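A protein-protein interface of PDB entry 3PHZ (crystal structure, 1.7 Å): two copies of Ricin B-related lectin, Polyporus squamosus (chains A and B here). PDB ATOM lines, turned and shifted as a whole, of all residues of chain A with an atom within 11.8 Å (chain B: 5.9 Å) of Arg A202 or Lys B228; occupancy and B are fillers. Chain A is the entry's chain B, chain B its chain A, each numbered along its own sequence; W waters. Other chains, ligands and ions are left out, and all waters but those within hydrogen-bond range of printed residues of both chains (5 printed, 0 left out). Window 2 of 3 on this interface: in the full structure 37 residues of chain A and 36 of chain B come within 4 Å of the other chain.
Among the printed residues, no Asp or Glu carboxylate lies within 4 Å of a Lys or Arg side-chain nitrogen of the other chain.
No position is printed for both chains. Of the 9 pairs that touch across the chains among the printed residues, none has its exchanged pair printed and touching as well.
Of chain B, only Asn B224, Phe B227, Lys B228 and Ala B229 come within 4 Å of Arg A202. Of chain A, only Arg A202 (3.3 Å) comes within 4 Å of Lys B228. No residue of chain A comes within 4 Å of Ala B65. No residue of chain A comes within 4 Å of Gly B68. Of chain A, only Thr A199, Arg A202 and Phe A206 come within 4 Å of Asn B224. Of chain A, only Ser A203 and Ile A205 come within 4 Å of Asn B230. Printed residues of chain B within 4 Å of Thr A199: Asn B224. Printed residues of chain B within 4 Å of Ile A205: Ala B229 and Asn B230. Of the printed residues of chain B, Ser A203 touches Asn B230. Of the printed residues of chain B, Phe A206 touches Asn B224 (3.6 Å). Cys A208 touches none of the printed residues of chain B. The nearest residue of chain B that does not touch Arg A202 is Gly B223 (4.4 Å). The nearest residue of chain A that does not touch Lys B228 is Ile A205 (6.2 Å). The nearest printed residue of chain B that does not touch Phe A206 is Gly B223 (6.2 Å).
The backbone carbonyl oxygen of Lys B228 sits at hydrogen-bond distance from the guanidinium group of Arg A202. The guanidinium group (NH2) of Arg A202 is in hydrogen-bond range of the side-chain amide oxygen (OD1) of Asn B224 (3.0 Å). The backbone carbonyl oxygen (O) of Ala B229 sits at hydrogen-bond distance from the guanidinium group (NH1) of Arg A202. The backbone carbonyl oxygen of Phe B227 is in hydrogen-bond range of the guanidinium group of Arg A202 (2.9 Å).
Asn B224 touches Thr A199. O of Ser A203 touches CB of Asn B230 (3.7 Å). Ile A205 touches Ala B229. CA of Asn B230 touches CG2 of Ile A205 (3.8 Å). Asn B224 touches Phe A206.
Water W4 lies within hydrogen-bond range of the backbone carbonyl oxygen (O) of Pro A200 (2.6 Å), the side-chain amide oxygen (OD1) of Asn B224 (2.7 Å) and the guanidinium group (NE) of Arg A202 (3.0 Å). Water W2 lies within hydrogen-bond range of O of Ile A205 and N of Asn B224. Water W5 bridges O of Lys B228 and NH1 of Arg A202. Water W3 bridges N of Ser A203 and ND2 of Asn B230. Water W1 bridges the backbone carbonyl oxygen of Lys B228 (2.9 Å) and the guanidinium group of Arg A202 (3.1 Å).
The backbone carbonyl oxygen (O) of Phe B66 lies within hydrogen-bond range of the backbone NH (N) of Lys B228, at 3.0 Å. NZ of Lys B228 is in hydrogen-bond range of O of Glu B225, at 3.0 Å. The backbone carbonyl oxygen (O) of Ala B65 lies within hydrogen-bond range of the backbone NH (N) of Ala B229 (3.1 Å). The backbone carbonyl oxygen (O) of Ala B65 sits at hydrogen-bond distance from the backbone NH (N) of Lys B228, at 3.2 Å. OD1 of Asn B230 is in hydrogen-bond range of NH1 of Arg B63, 3.1 Å away.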
ATOM      1  N   LEU A 196     -34.956   7.542 -21.207  1.00  0.00           N
ATOM      2  CA  LEU A 196     -34.610   7.488 -22.641  1.00  0.00           C
ATOM      3  C   LEU A 196     -34.335   8.904 -23.197  1.00  0.00           C
ATOM      4  O   LEU A 196     -33.484   9.080 -24.076  1.00  0.00           O
ATOM      5  CB  LEU A 196     -35.694   6.785 -23.459  1.00  0.00           C
ATOM      6  CG  LEU A 196     -35.709   5.253 -23.180  1.00  0.00           C
ATOM      7  CD1 LEU A 196     -36.939   4.692 -23.883  1.00  0.00           C
ATOM      8  CD2 LEU A 196     -34.452   4.525 -23.721  1.00  0.00           C
ATOM      9  N   GLY A 197     -35.000   9.906 -22.624  1.00  0.00           N
ATOM     10  CA  GLY A 197     -34.858  11.297 -23.167  1.00  0.00           C
ATOM     11  C   GLY A 197     -33.462  11.811 -22.957  1.00  0.00           C
ATOM     12  O   GLY A 197     -33.032  12.720 -23.688  1.00  0.00           O
ATOM     13  N   SER A 198     -32.744  11.259 -21.964  1.00  0.00           N
ATOM     14  CA  SER A 198     -31.327  11.649 -21.783  1.00  0.00           C
ATOM     15  C   SER A 198     -30.300  10.585 -22.242  1.00  0.00           C
ATOM     16  O   SER A 198     -29.132  10.638 -21.897  1.00  0.00           O
ATOM     17  CB  SER A 198     -31.087  12.099 -20.338  1.00  0.00           C
ATOM     18  OG  SER A 198     -31.404  11.047 -19.483  1.00  0.00           O
ATOM     19  N   THR A 199     -30.762   9.627 -23.039  1.00  0.00           N
ATOM     20  CA  THR A 199     -29.904   8.590 -23.561  1.00  0.00           C
ATOM     21  C   THR A 199     -29.619   8.937 -25.048  1.00  0.00           C
ATOM     22  O   THR A 199     -30.541   8.917 -25.867  1.00  0.00           O
ATOM     23  CB  THR A 199     -30.583   7.206 -23.449  1.00  0.00           C
ATOM     24  OG1 THR A 199     -30.987   6.980 -22.074  1.00  0.00           O
ATOM     25  CG2 THR A 199     -29.638   6.042 -23.915  1.00  0.00           C
ATOM     26  N   PRO A 200     -28.347   9.178 -25.402  1.00  0.00           N
ATOM     27  CA  PRO A 200     -28.046   9.554 -26.782  1.00  0.00           C
ATOM     28  C   PRO A 200     -28.213   8.366 -27.711  1.00  0.00           C
ATOM     29  O   PRO A 200     -27.856   7.251 -27.340  1.00  0.00           O
ATOM     30  CB  PRO A 200     -26.552   9.997 -26.735  1.00  0.00           C
ATOM     31  CG  PRO A 200     -26.294  10.317 -25.222  1.00  0.00           C
ATOM     32  CD  PRO A 200     -27.177   9.318 -24.506  1.00  0.00           C
ATOM     33  N   TRP A 201     -28.803   8.609 -28.887  1.00  0.00           N
ATOM     34  CA  TRP A 201     -28.780   7.657 -29.987  1.00  0.00           C
ATOM     35  C   TRP A 201     -27.320   7.432 -30.392  1.00  0.00           C
ATOM     36  O   TRP A 201     -26.536   8.401 -30.524  1.00  0.00           O
ATOM     37  CB  TRP A 201     -29.556   8.236 -31.178  1.00  0.00           C
ATOM     38  CG  TRP A 201     -29.564   7.350 -32.382  1.00  0.00           C
ATOM     39  CD1 TRP A 201     -30.514   6.413 -32.735  1.00  0.00           C
ATOM     40  CD2 TRP A 201     -28.586   7.359 -33.428  1.00  0.00           C
ATOM     41  NE1 TRP A 201     -30.161   5.816 -33.955  1.00  0.00           N
ATOM     42  CE2 TRP A 201     -28.987   6.391 -34.394  1.00  0.00           C
ATOM     43  CE3 TRP A 201     -27.423   8.124 -33.657  1.00  0.00           C
ATOM     44  CZ2 TRP A 201     -28.224   6.130 -35.562  1.00  0.00           C
ATOM     45  CZ3 TRP A 201     -26.647   7.872 -34.844  1.00  0.00           C
ATOM     46  CH2 TRP A 201     -27.060   6.874 -35.765  1.00  0.00           C
ATOM     47  N   ARG A 202     -26.963   6.165 -30.614  1.00  0.00           N
ATOM     48  CA  ARG A 202     -25.685   5.786 -31.234  1.00  0.00           C
ATOM     49  C   ARG A 202     -25.855   4.671 -32.241  1.00  0.00           C
ATOM     50  O   ARG A 202     -26.607   3.729 -32.010  1.00  0.00           O
ATOM     51  CB  ARG A 202     -24.680   5.396 -30.142  1.00  0.00           C
ATOM     52  CG  ARG A 202     -24.366   6.556 -29.158  1.00  0.00           C
ATOM     53  CD  ARG A 202     -23.153   6.164 -28.286  1.00  0.00           C
ATOM     54  NE  ARG A 202     -23.488   5.111 -27.341  1.00  0.00           N
ATOM     55  CZ  ARG A 202     -22.642   4.143 -26.993  1.00  0.00           C
ATOM     56  NH1 ARG A 202     -21.438   4.009 -27.567  1.00  0.00           N
ATOM     57  NH2 ARG A 202     -22.974   3.287 -26.040  1.00  0.00           N
ATOM     58  N   SER A 203     -25.149   4.783 -33.364  1.00  0.00           N
ATOM     59  CA  SER A 203     -25.303   3.854 -34.459  1.00  0.00           C
ATOM     60  C   SER A 203     -25.104   2.406 -34.001  1.00  0.00           C
ATOM     61  O   SER A 203     -24.080   2.070 -33.421  1.00  0.00           O
ATOM     62  CB  SER A 203     -24.290   4.160 -35.562  1.00  0.00           C
ATOM     63  OG  SER A 203     -24.625   3.278 -36.639  1.00  0.00           O
ATOM     64  N   GLU A 204     -26.120   1.582 -34.242  1.00  0.00           N
ATOM     65  CA  GLU A 204     -26.226   0.144 -33.822  1.00  0.00           C
ATOM     66  C   GLU A 204     -26.253  -0.156 -32.357  1.00  0.00           C
ATOM     67  O   GLU A 204     -27.083  -0.960 -31.921  1.00  0.00           O
ATOM     68  CB  GLU A 204     -25.200  -0.773 -34.530  1.00  0.00           C
ATOM     69  CG  GLU A 204     -25.220  -0.527 -36.083  1.00  0.00           C
ATOM     70  CD  GLU A 204     -24.521  -1.622 -36.887  1.00  0.00           C
ATOM     71  OE1 GLU A 204     -24.238  -2.715 -36.377  1.00  0.00           O
ATOM     72  OE2 GLU A 204     -24.382  -1.426 -38.113  1.00  0.00           O
ATOM     73  N   ILE A 205     -25.358   0.472 -31.601  1.00  0.00           N
ATOM     74  CA  ILE A 205     -25.185   0.121 -30.197  1.00  0.00           C
ATOM     75  C   ILE A 205     -26.305   0.670 -29.297  1.00  0.00           C
ATOM     76  O   ILE A 205     -26.645   0.053 -28.262  1.00  0.00           O
ATOM     77  CB  ILE A 205     -23.777   0.541 -29.707  1.00  0.00           C
ATOM     78  CG1 ILE A 205     -23.441  -0.082 -28.329  1.00  0.00           C
ATOM     79  CG2 ILE A 205     -23.629   2.042 -29.715  1.00  0.00           C
ATOM     80  CD1 ILE A 205     -23.394  -1.585 -28.408  1.00  0.00           C
ATOM     81  N   PHE A 206     -26.923   1.789 -29.686  1.00  0.00           N
ATOM     82  CA  PHE A 206     -28.173   2.131 -29.014  1.00  0.00           C
ATOM     83  C   PHE A 206     -29.015   2.896 -30.030  1.00  0.00           C
ATOM     84  O   PHE A 206     -29.037   4.122 -30.054  1.00  0.00           O
ATOM     85  CB  PHE A 206     -27.942   2.880 -27.705  1.00  0.00           C
ATOM     86  CG  PHE A 206     -29.127   2.745 -26.789  1.00  0.00           C
ATOM     87  CD1 PHE A 206     -29.388   1.530 -26.127  1.00  0.00           C
ATOM     88  CD2 PHE A 206     -30.096   3.765 -26.758  1.00  0.00           C
ATOM     89  CE1 PHE A 206     -30.535   1.407 -25.299  1.00  0.00           C
ATOM     90  CE2 PHE A 206     -31.261   3.638 -25.977  1.00  0.00           C
ATOM     91  CZ  PHE A 206     -31.491   2.445 -25.257  1.00  0.00           C
ATOM     92  N   ASP A 207     -29.626   2.110 -30.904  1.00  0.00           N
ATOM     93  CA  ASP A 207     -30.251   2.603 -32.089  1.00  0.00           C
ATOM     94  C   ASP A 207     -31.796   2.727 -31.913  1.00  0.00           C
ATOM     95  O   ASP A 207     -32.339   2.584 -30.798  1.00  0.00           O
ATOM     96  CB  ASP A 207     -29.899   1.662 -33.269  1.00  0.00           C
ATOM     97  CG  ASP A 207     -29.724   2.428 -34.621  1.00  0.00           C
ATOM     98  OD1 ASP A 207     -30.686   3.166 -35.047  1.00  0.00           O
ATOM     99  OD2 ASP A 207     -28.641   2.220 -35.303  1.00  0.00           O
ATOM    100  N   CYS A 208     -32.515   3.044 -32.995  1.00  0.00           N
ATOM    101  CA  CYS A 208     -33.944   3.400 -32.807  1.00  0.00           C
ATOM    102  C   CYS A 208     -34.752   2.220 -32.262  1.00  0.00           C
ATOM    103  O   CYS A 208     -35.683   2.421 -31.494  1.00  0.00           O
ATOM    104  CB  CYS A 208     -34.639   3.858 -34.091  1.00  0.00           C
ATOM    105  SG  CYS A 208     -33.845   5.324 -34.637  1.00  0.00           S
ATOM    106  N   ASP A 209     -34.440   1.025 -32.734  1.00  0.00           N
ATOM    107  CA  ASP A 209     -35.120  -0.172 -32.212  1.00  0.00           C
ATOM    108  C   ASP A 209     -34.904  -0.335 -30.693  1.00  0.00           C
ATOM    109  O   ASP A 209     -35.812  -0.817 -30.009  1.00  0.00           O
ATOM    110  CB  ASP A 209     -34.712  -1.458 -32.944  1.00  0.00           C
ATOM    111  CG  ASP A 209     -33.207  -1.786 -32.848  1.00  0.00           C
ATOM    112  OD1 ASP A 209     -32.303  -0.883 -32.744  1.00  0.00           O
ATOM    113  OD2 ASP A 209     -32.955  -3.024 -32.876  1.00  0.00           O
ATOM    114  N   ASP A 210     -33.720   0.038 -30.194  1.00  0.00           N
ATOM    115  CA  ASP A 210     -33.439  -0.076 -28.771  1.00  0.00           C
ATOM    116  C   ASP A 210     -34.285   0.899 -28.000  1.00  0.00           C
ATOM    117  O   ASP A 210     -34.874   0.541 -26.981  1.00  0.00           O
ATOM    118  CB  ASP A 210     -31.970   0.110 -28.505  1.00  0.00           C
ATOM    119  CG  ASP A 210     -31.159  -0.934 -29.223  1.00  0.00           C
ATOM    120  OD1 ASP A 210     -31.535  -2.132 -29.184  1.00  0.00           O
ATOM    121  OD2 ASP A 210     -30.067  -0.568 -29.739  1.00  0.00           O
ATOM    122  N   PHE A 211     -34.490   2.104 -28.532  1.00  0.00           N
ATOM    123  CA  PHE A 211     -35.365   3.060 -27.814  1.00  0.00           C
ATOM    124  C   PHE A 211     -36.790   2.499 -27.773  1.00  0.00           C
ATOM    125  O   PHE A 211     -37.476   2.582 -26.742  1.00  0.00           O
ATOM    126  CB  PHE A 211     -35.405   4.421 -28.538  1.00  0.00           C
ATOM    127  CG  PHE A 211     -34.199   5.282 -28.290  1.00  0.00           C
ATOM    128  CD1 PHE A 211     -34.178   6.198 -27.219  1.00  0.00           C
ATOM    129  CD2 PHE A 211     -33.053   5.144 -29.099  1.00  0.00           C
ATOM    130  CE1 PHE A 211     -33.070   6.999 -26.959  1.00  0.00           C
ATOM    131  CE2 PHE A 211     -31.920   5.947 -28.859  1.00  0.00           C
ATOM    132  CZ  PHE A 211     -31.913   6.883 -27.773  1.00  0.00           C
ATOM    133  N   ALA A 212     -37.263   1.947 -28.910  1.00  0.00           N
ATOM    134  CA  ALA A 212     -38.665   1.548 -28.957  1.00  0.00           C
ATOM    135  C   ALA A 212     -38.886   0.284 -28.103  1.00  0.00           C
ATOM    136  O   ALA A 212     -39.950   0.123 -27.525  1.00  0.00           O
ATOM    137  CB  ALA A 212     -39.114   1.258 -30.406  1.00  0.00           C
ATOM    138  N   ALA A 247     -34.102   4.003 -42.213  1.00  0.00           N
ATOM    139  CA  ALA A 247     -35.080   3.269 -41.345  1.00  0.00           C
ATOM    140  C   ALA A 247     -35.278   4.025 -40.034  1.00  0.00           C
ATOM    141  O   ALA A 247     -34.424   4.862 -39.649  1.00  0.00           O
ATOM    142  CB  ALA A 247     -34.604   1.893 -41.069  1.00  0.00           C
ATOM    143  N   HIS A 248     -36.411   3.777 -39.370  1.00  0.00           N
ATOM    144  CA  HIS A 248     -36.631   4.312 -38.037  1.00  0.00           C
ATOM    145  C   HIS A 248     -37.545   3.348 -37.280  1.00  0.00           C
ATOM    146  O   HIS A 248     -38.227   2.540 -37.883  1.00  0.00           O
ATOM    147  CB  HIS A 248     -37.309   5.679 -38.076  1.00  0.00           C
ATOM    148  CG  HIS A 248     -36.970   6.558 -36.900  1.00  0.00           C
ATOM    149  ND1 HIS A 248     -35.810   7.311 -36.841  1.00  0.00           N
ATOM    150  CD2 HIS A 248     -37.654   6.841 -35.760  1.00  0.00           C
ATOM    151  CE1 HIS A 248     -35.790   8.009 -35.711  1.00  0.00           C
ATOM    152  NE2 HIS A 248     -36.898   7.736 -35.037  1.00  0.00           N
ATOM    153  N   ALA A 249     -37.579   3.504 -35.963  1.00  0.00           N
ATOM    154  CA  ALA A 249     -38.489   2.709 -35.152  1.00  0.00           C
ATOM    155  C   ALA A 249     -39.235   3.632 -34.240  1.00  0.00           C
ATOM    156  O   ALA A 249     -38.633   4.601 -33.704  1.00  0.00           O
ATOM    157  CB  ALA A 249     -37.745   1.666 -34.263  1.00  0.00           C
ATOM    158  N   GLU A 266     -42.313   8.933 -30.407  1.00  0.00           N
ATOM    159  CA  GLU A 266     -40.855   8.874 -30.648  1.00  0.00           C
ATOM    160  C   GLU A 266     -40.174   8.738 -29.280  1.00  0.00           C
ATOM    161  O   GLU A 266     -40.038   9.715 -28.516  1.00  0.00           O
ATOM    162  CB  GLU A 266     -40.407  10.190 -31.359  1.00  0.00           C
ATOM    163  CG  GLU A 266     -38.904  10.461 -31.384  1.00  0.00           C
ATOM    164  CD  GLU A 266     -38.118   9.316 -32.037  1.00  0.00           C
ATOM    165  OE1 GLU A 266     -37.751   8.336 -31.338  1.00  0.00           O
ATOM    166  OE2 GLU A 266     -37.833   9.408 -33.260  1.00  0.00           O
ATOM    167  N   PRO A 267     -39.729   7.518 -28.956  1.00  0.00           N
ATOM    168  CA  PRO A 267     -39.196   7.347 -27.633  1.00  0.00           C
ATOM    169  C   PRO A 267     -37.814   8.003 -27.420  1.00  0.00           C
ATOM    170  O   PRO A 267     -37.354   8.079 -26.268  1.00  0.00           O
ATOM    171  CB  PRO A 267     -39.142   5.792 -27.495  1.00  0.00           C
ATOM    172  CG  PRO A 267     -38.863   5.330 -28.908  1.00  0.00           C
ATOM    173  CD  PRO A 267     -39.784   6.259 -29.724  1.00  0.00           C
ATOM    174  N   GLN A 268     -37.161   8.517 -28.475  1.00  0.00           N
ATOM    175  CA  GLN A 268     -35.962   9.327 -28.225  1.00  0.00           C
ATOM    176  C   GLN A 268     -36.223  10.687 -27.579  1.00  0.00           C
ATOM    177  O   GLN A 268     -35.340  11.227 -26.912  1.00  0.00           O
ATOM    178  CB  GLN A 268     -35.243   9.560 -29.547  1.00  0.00           C
ATOM    179  CG  GLN A 268     -34.576   8.315 -30.035  1.00  0.00           C
ATOM    180  CD  GLN A 268     -33.810   8.505 -31.363  1.00  0.00           C
ATOM    181  OE1 GLN A 268     -34.054   7.800 -32.336  1.00  0.00           O
ATOM    182  NE2 GLN A 268     -32.873   9.430 -31.379  1.00  0.00           N
ATOM    183  N   ARG B  63     -10.354  -1.032 -32.791  1.00  0.00           N
ATOM    184  CA  ARG B  63     -10.876  -0.163 -31.787  1.00  0.00           C
ATOM    185  C   ARG B  63     -11.240  -0.989 -30.549  1.00  0.00           C
ATOM    186  O   ARG B  63     -11.783  -2.099 -30.652  1.00  0.00           O
ATOM    187  CB  ARG B  63     -12.182   0.497 -32.348  1.00  0.00           C
ATOM    188  CG  ARG B  63     -12.784   1.523 -31.466  1.00  0.00           C
ATOM    189  CD  ARG B  63     -14.020   2.209 -32.167  1.00  0.00           C
ATOM    190  NE  ARG B  63     -14.337   3.375 -31.378  1.00  0.00           N
ATOM    191  CZ  ARG B  63     -15.395   4.161 -31.557  1.00  0.00           C
ATOM    192  NH1 ARG B  63     -16.292   3.886 -32.515  1.00  0.00           N
ATOM    193  NH2 ARG B  63     -15.508   5.251 -30.807  1.00  0.00           N
ATOM    194  N   ASN B  64     -10.983  -0.423 -29.386  1.00  0.00           N
ATOM    195  CA  ASN B  64     -11.378  -1.108 -28.167  1.00  0.00           C
ATOM    196  C   ASN B  64     -12.881  -0.872 -27.998  1.00  0.00           C
ATOM    197  O   ASN B  64     -13.320   0.271 -27.893  1.00  0.00           O
ATOM    198  CB  ASN B  64     -10.612  -0.487 -26.978  1.00  0.00           C
ATOM    199  CG  ASN B  64     -10.705  -1.384 -25.728  1.00  0.00           C
ATOM    200  OD1 ASN B  64     -11.533  -1.109 -24.840  1.00  0.00           O
ATOM    201  ND2 ASN B  64      -9.988  -2.561 -25.748  1.00  0.00           N
ATOM    202  N   ALA B  65     -13.683  -1.954 -27.953  1.00  0.00           N
ATOM    203  CA  ALA B  65     -15.149  -1.807 -27.998  1.00  0.00           C
ATOM    204  C   ALA B  65     -15.590  -1.120 -26.690  1.00  0.00           C
ATOM    205  O   ALA B  65     -16.503  -0.309 -26.659  1.00  0.00           O
ATOM    206  CB  ALA B  65     -15.833  -3.203 -28.156  1.00  0.00           C
ATOM    207  N   PHE B  66     -14.923  -1.512 -25.590  1.00  0.00           N
ATOM    208  CA  PHE B  66     -15.237  -0.998 -24.259  1.00  0.00           C
ATOM    209  C   PHE B  66     -14.838   0.450 -24.130  1.00  0.00           C
ATOM    210  O   PHE B  66     -15.689   1.285 -23.821  1.00  0.00           O
ATOM    211  CB  PHE B  66     -14.534  -1.868 -23.215  1.00  0.00           C
ATOM    212  CG  PHE B  66     -14.783  -1.428 -21.781  1.00  0.00           C
ATOM    213  CD1 PHE B  66     -15.996  -1.736 -21.187  1.00  0.00           C
ATOM    214  CD2 PHE B  66     -13.803  -0.731 -21.050  1.00  0.00           C
ATOM    215  CE1 PHE B  66     -16.260  -1.371 -19.853  1.00  0.00           C
ATOM    216  CE2 PHE B  66     -14.082  -0.338 -19.699  1.00  0.00           C
ATOM    217  CZ  PHE B  66     -15.303  -0.661 -19.130  1.00  0.00           C
ATOM    218  N   ALA B  67     -13.565   0.782 -24.336  1.00  0.00           N
ATOM    219  CA  ALA B  67     -13.105   2.175 -24.054  1.00  0.00           C
ATOM    220  C   ALA B  67     -13.407   3.144 -25.185  1.00  0.00           C
ATOM    221  O   ALA B  67     -13.430   4.333 -24.975  1.00  0.00           O
ATOM    222  CB  ALA B  67     -11.618   2.153 -23.760  1.00  0.00           C
ATOM    223  N   GLY B  68     -13.670   2.620 -26.375  1.00  0.00           N
ATOM    224  CA  GLY B  68     -13.912   3.414 -27.592  1.00  0.00           C
ATOM    225  C   GLY B  68     -12.666   3.968 -28.271  1.00  0.00           C
ATOM    226  O   GLY B  68     -12.755   4.563 -29.313  1.00  0.00           O
ATOM    227  N   GLY B 223     -25.421  -3.063 -23.122  1.00  0.00           N
ATOM    228  CA  GLY B 223     -24.433  -2.757 -24.140  1.00  0.00           C
ATOM    229  C   GLY B 223     -24.180  -1.244 -24.182  1.00  0.00           C
ATOM    230  O   GLY B 223     -23.040  -0.810 -24.360  1.00  0.00           O
ATOM    231  N   ASN B 224     -25.238  -0.450 -24.019  1.00  0.00           N
ATOM    232  CA  ASN B 224     -25.112   0.976 -24.137  1.00  0.00           C
ATOM    233  C   ASN B 224     -24.228   1.506 -22.990  1.00  0.00           C
ATOM    234  O   ASN B 224     -23.391   2.413 -23.159  1.00  0.00           O
ATOM    235  CB  ASN B 224     -26.486   1.651 -24.024  1.00  0.00           C
ATOM    236  CG  ASN B 224     -26.377   3.185 -24.078  1.00  0.00           C
ATOM    237  OD1 ASN B 224     -25.789   3.754 -25.007  1.00  0.00           O
ATOM    238  ND2 ASN B 224     -26.957   3.863 -23.077  1.00  0.00           N
ATOM    239  N   GLU B 225     -24.434   0.938 -21.833  1.00  0.00           N
ATOM    240  CA  GLU B 225     -23.732   1.432 -20.618  1.00  0.00           C
ATOM    241  C   GLU B 225     -22.284   1.013 -20.633  1.00  0.00           C
ATOM    242  O   GLU B 225     -21.453   1.685 -19.991  1.00  0.00           O
ATOM    243  CB  GLU B 225     -24.395   0.850 -19.386  1.00  0.00           C
ATOM    244  CG  GLU B 225     -25.810   1.442 -19.186  1.00  0.00           C
ATOM    245  CD  GLU B 225     -26.676   0.589 -18.267  1.00  0.00           C
ATOM    246  OE1 GLU B 225     -26.186  -0.471 -17.779  1.00  0.00           O
ATOM    247  OE2 GLU B 225     -27.866   0.937 -18.118  1.00  0.00           O
ATOM    248  N   ASN B 226     -21.982  -0.108 -21.293  1.00  0.00           N
ATOM    249  CA  ASN B 226     -20.637  -0.672 -21.214  1.00  0.00           C
ATOM    250  C   ASN B 226     -19.700  -0.409 -22.400  1.00  0.00           C
ATOM    251  O   ASN B 226     -18.471  -0.437 -22.251  1.00  0.00           O
ATOM    252  CB  ASN B 226     -20.719  -2.167 -20.903  1.00  0.00           C
ATOM    253  CG  ASN B 226     -21.076  -2.419 -19.443  1.00  0.00           C
ATOM    254  OD1 ASN B 226     -20.194  -2.298 -18.565  1.00  0.00           O
ATOM    255  ND2 ASN B 226     -22.359  -2.651 -19.148  1.00  0.00           N
ATOM    256  N   PHE B 227     -20.223  -0.190 -23.578  1.00  0.00           N
ATOM    257  CA  PHE B 227     -19.363  -0.027 -24.751  1.00  0.00           C
ATOM    258  C   PHE B 227     -19.372   1.396 -25.282  1.00  0.00           C
ATOM    259  O   PHE B 227     -20.426   1.916 -25.657  1.00  0.00           O
ATOM    260  CB  PHE B 227     -19.837  -0.989 -25.848  1.00  0.00           C
ATOM    261  CG  PHE B 227     -19.714  -2.446 -25.434  1.00  0.00           C
ATOM    262  CD1 PHE B 227     -18.447  -3.025 -25.310  1.00  0.00           C
ATOM    263  CD2 PHE B 227     -20.841  -3.191 -25.163  1.00  0.00           C
ATOM    264  CE1 PHE B 227     -18.330  -4.361 -24.902  1.00  0.00           C
ATOM    265  CE2 PHE B 227     -20.766  -4.559 -24.772  1.00  0.00           C
ATOM    266  CZ  PHE B 227     -19.463  -5.132 -24.625  1.00  0.00           C
ATOM    267  N   LYS B 228     -18.220   2.025 -25.277  1.00  0.00           N
ATOM    268  CA  LYS B 228     -18.099   3.413 -25.781  1.00  0.00           C
ATOM    269  C   LYS B 228     -17.985   3.444 -27.286  1.00  0.00           C
ATOM    270  O   LYS B 228     -18.240   4.489 -27.903  1.00  0.00           O
ATOM    271  CB  LYS B 228     -16.920   4.129 -25.111  1.00  0.00           C
ATOM    272  CG  LYS B 228     -17.133   4.299 -23.529  1.00  0.00           C
ATOM    273  CD  LYS B 228     -18.379   5.097 -23.119  1.00  0.00           C
ATOM    274  CE  LYS B 228     -18.755   4.990 -21.538  1.00  0.00           C
ATOM    275  NZ  LYS B 228     -19.360   3.664 -20.987  1.00  0.00           N
ATOM    276  N   ALA B 229     -17.574   2.325 -27.882  1.00  0.00           N
ATOM    277  CA  ALA B 229     -17.546   2.204 -29.357  1.00  0.00           C
ATOM    278  C   ALA B 229     -18.972   2.126 -29.891  1.00  0.00           C
ATOM    279  O   ALA B 229     -19.904   1.731 -29.165  1.00  0.00           O
ATOM    280  CB  ALA B 229     -16.737   0.980 -29.820  1.00  0.00           C
ATOM    281  N   ASN B 230     -19.159   2.524 -31.146  1.00  0.00           N
ATOM    282  CA  ASN B 230     -20.420   2.285 -31.803  1.00  0.00           C
ATOM    283  C   ASN B 230     -20.188   1.377 -32.999  1.00  0.00           C
ATOM    284  O   ASN B 230     -19.104   0.821 -33.176  1.00  0.00           O
ATOM    285  CB  ASN B 230     -21.014   3.640 -32.184  1.00  0.00           C
ATOM    286  CG  ASN B 230     -20.227   4.325 -33.297  1.00  0.00           C
ATOM    287  OD1 ASN B 230     -19.140   3.872 -33.698  1.00  0.00           O
ATOM    288  ND2 ASN B 230     -20.792   5.422 -33.846  1.00  0.00           N
HETATM  289  O   HOH W   1     -20.150   5.721 -29.758  1.00  0.00           O
HETATM  290  O   HOH W   2     -26.450  -2.112 -26.744  1.00  0.00           O
HETATM  291  O   HOH W   3     -23.353   6.929 -33.637  1.00  0.00           O
HETATM  292  O   HOH W   4     -25.884   6.226 -25.980  1.00  0.00           O
HETATM  293  O   HOH W   5     -19.478   6.619 -26.574  1.00  0.00           O
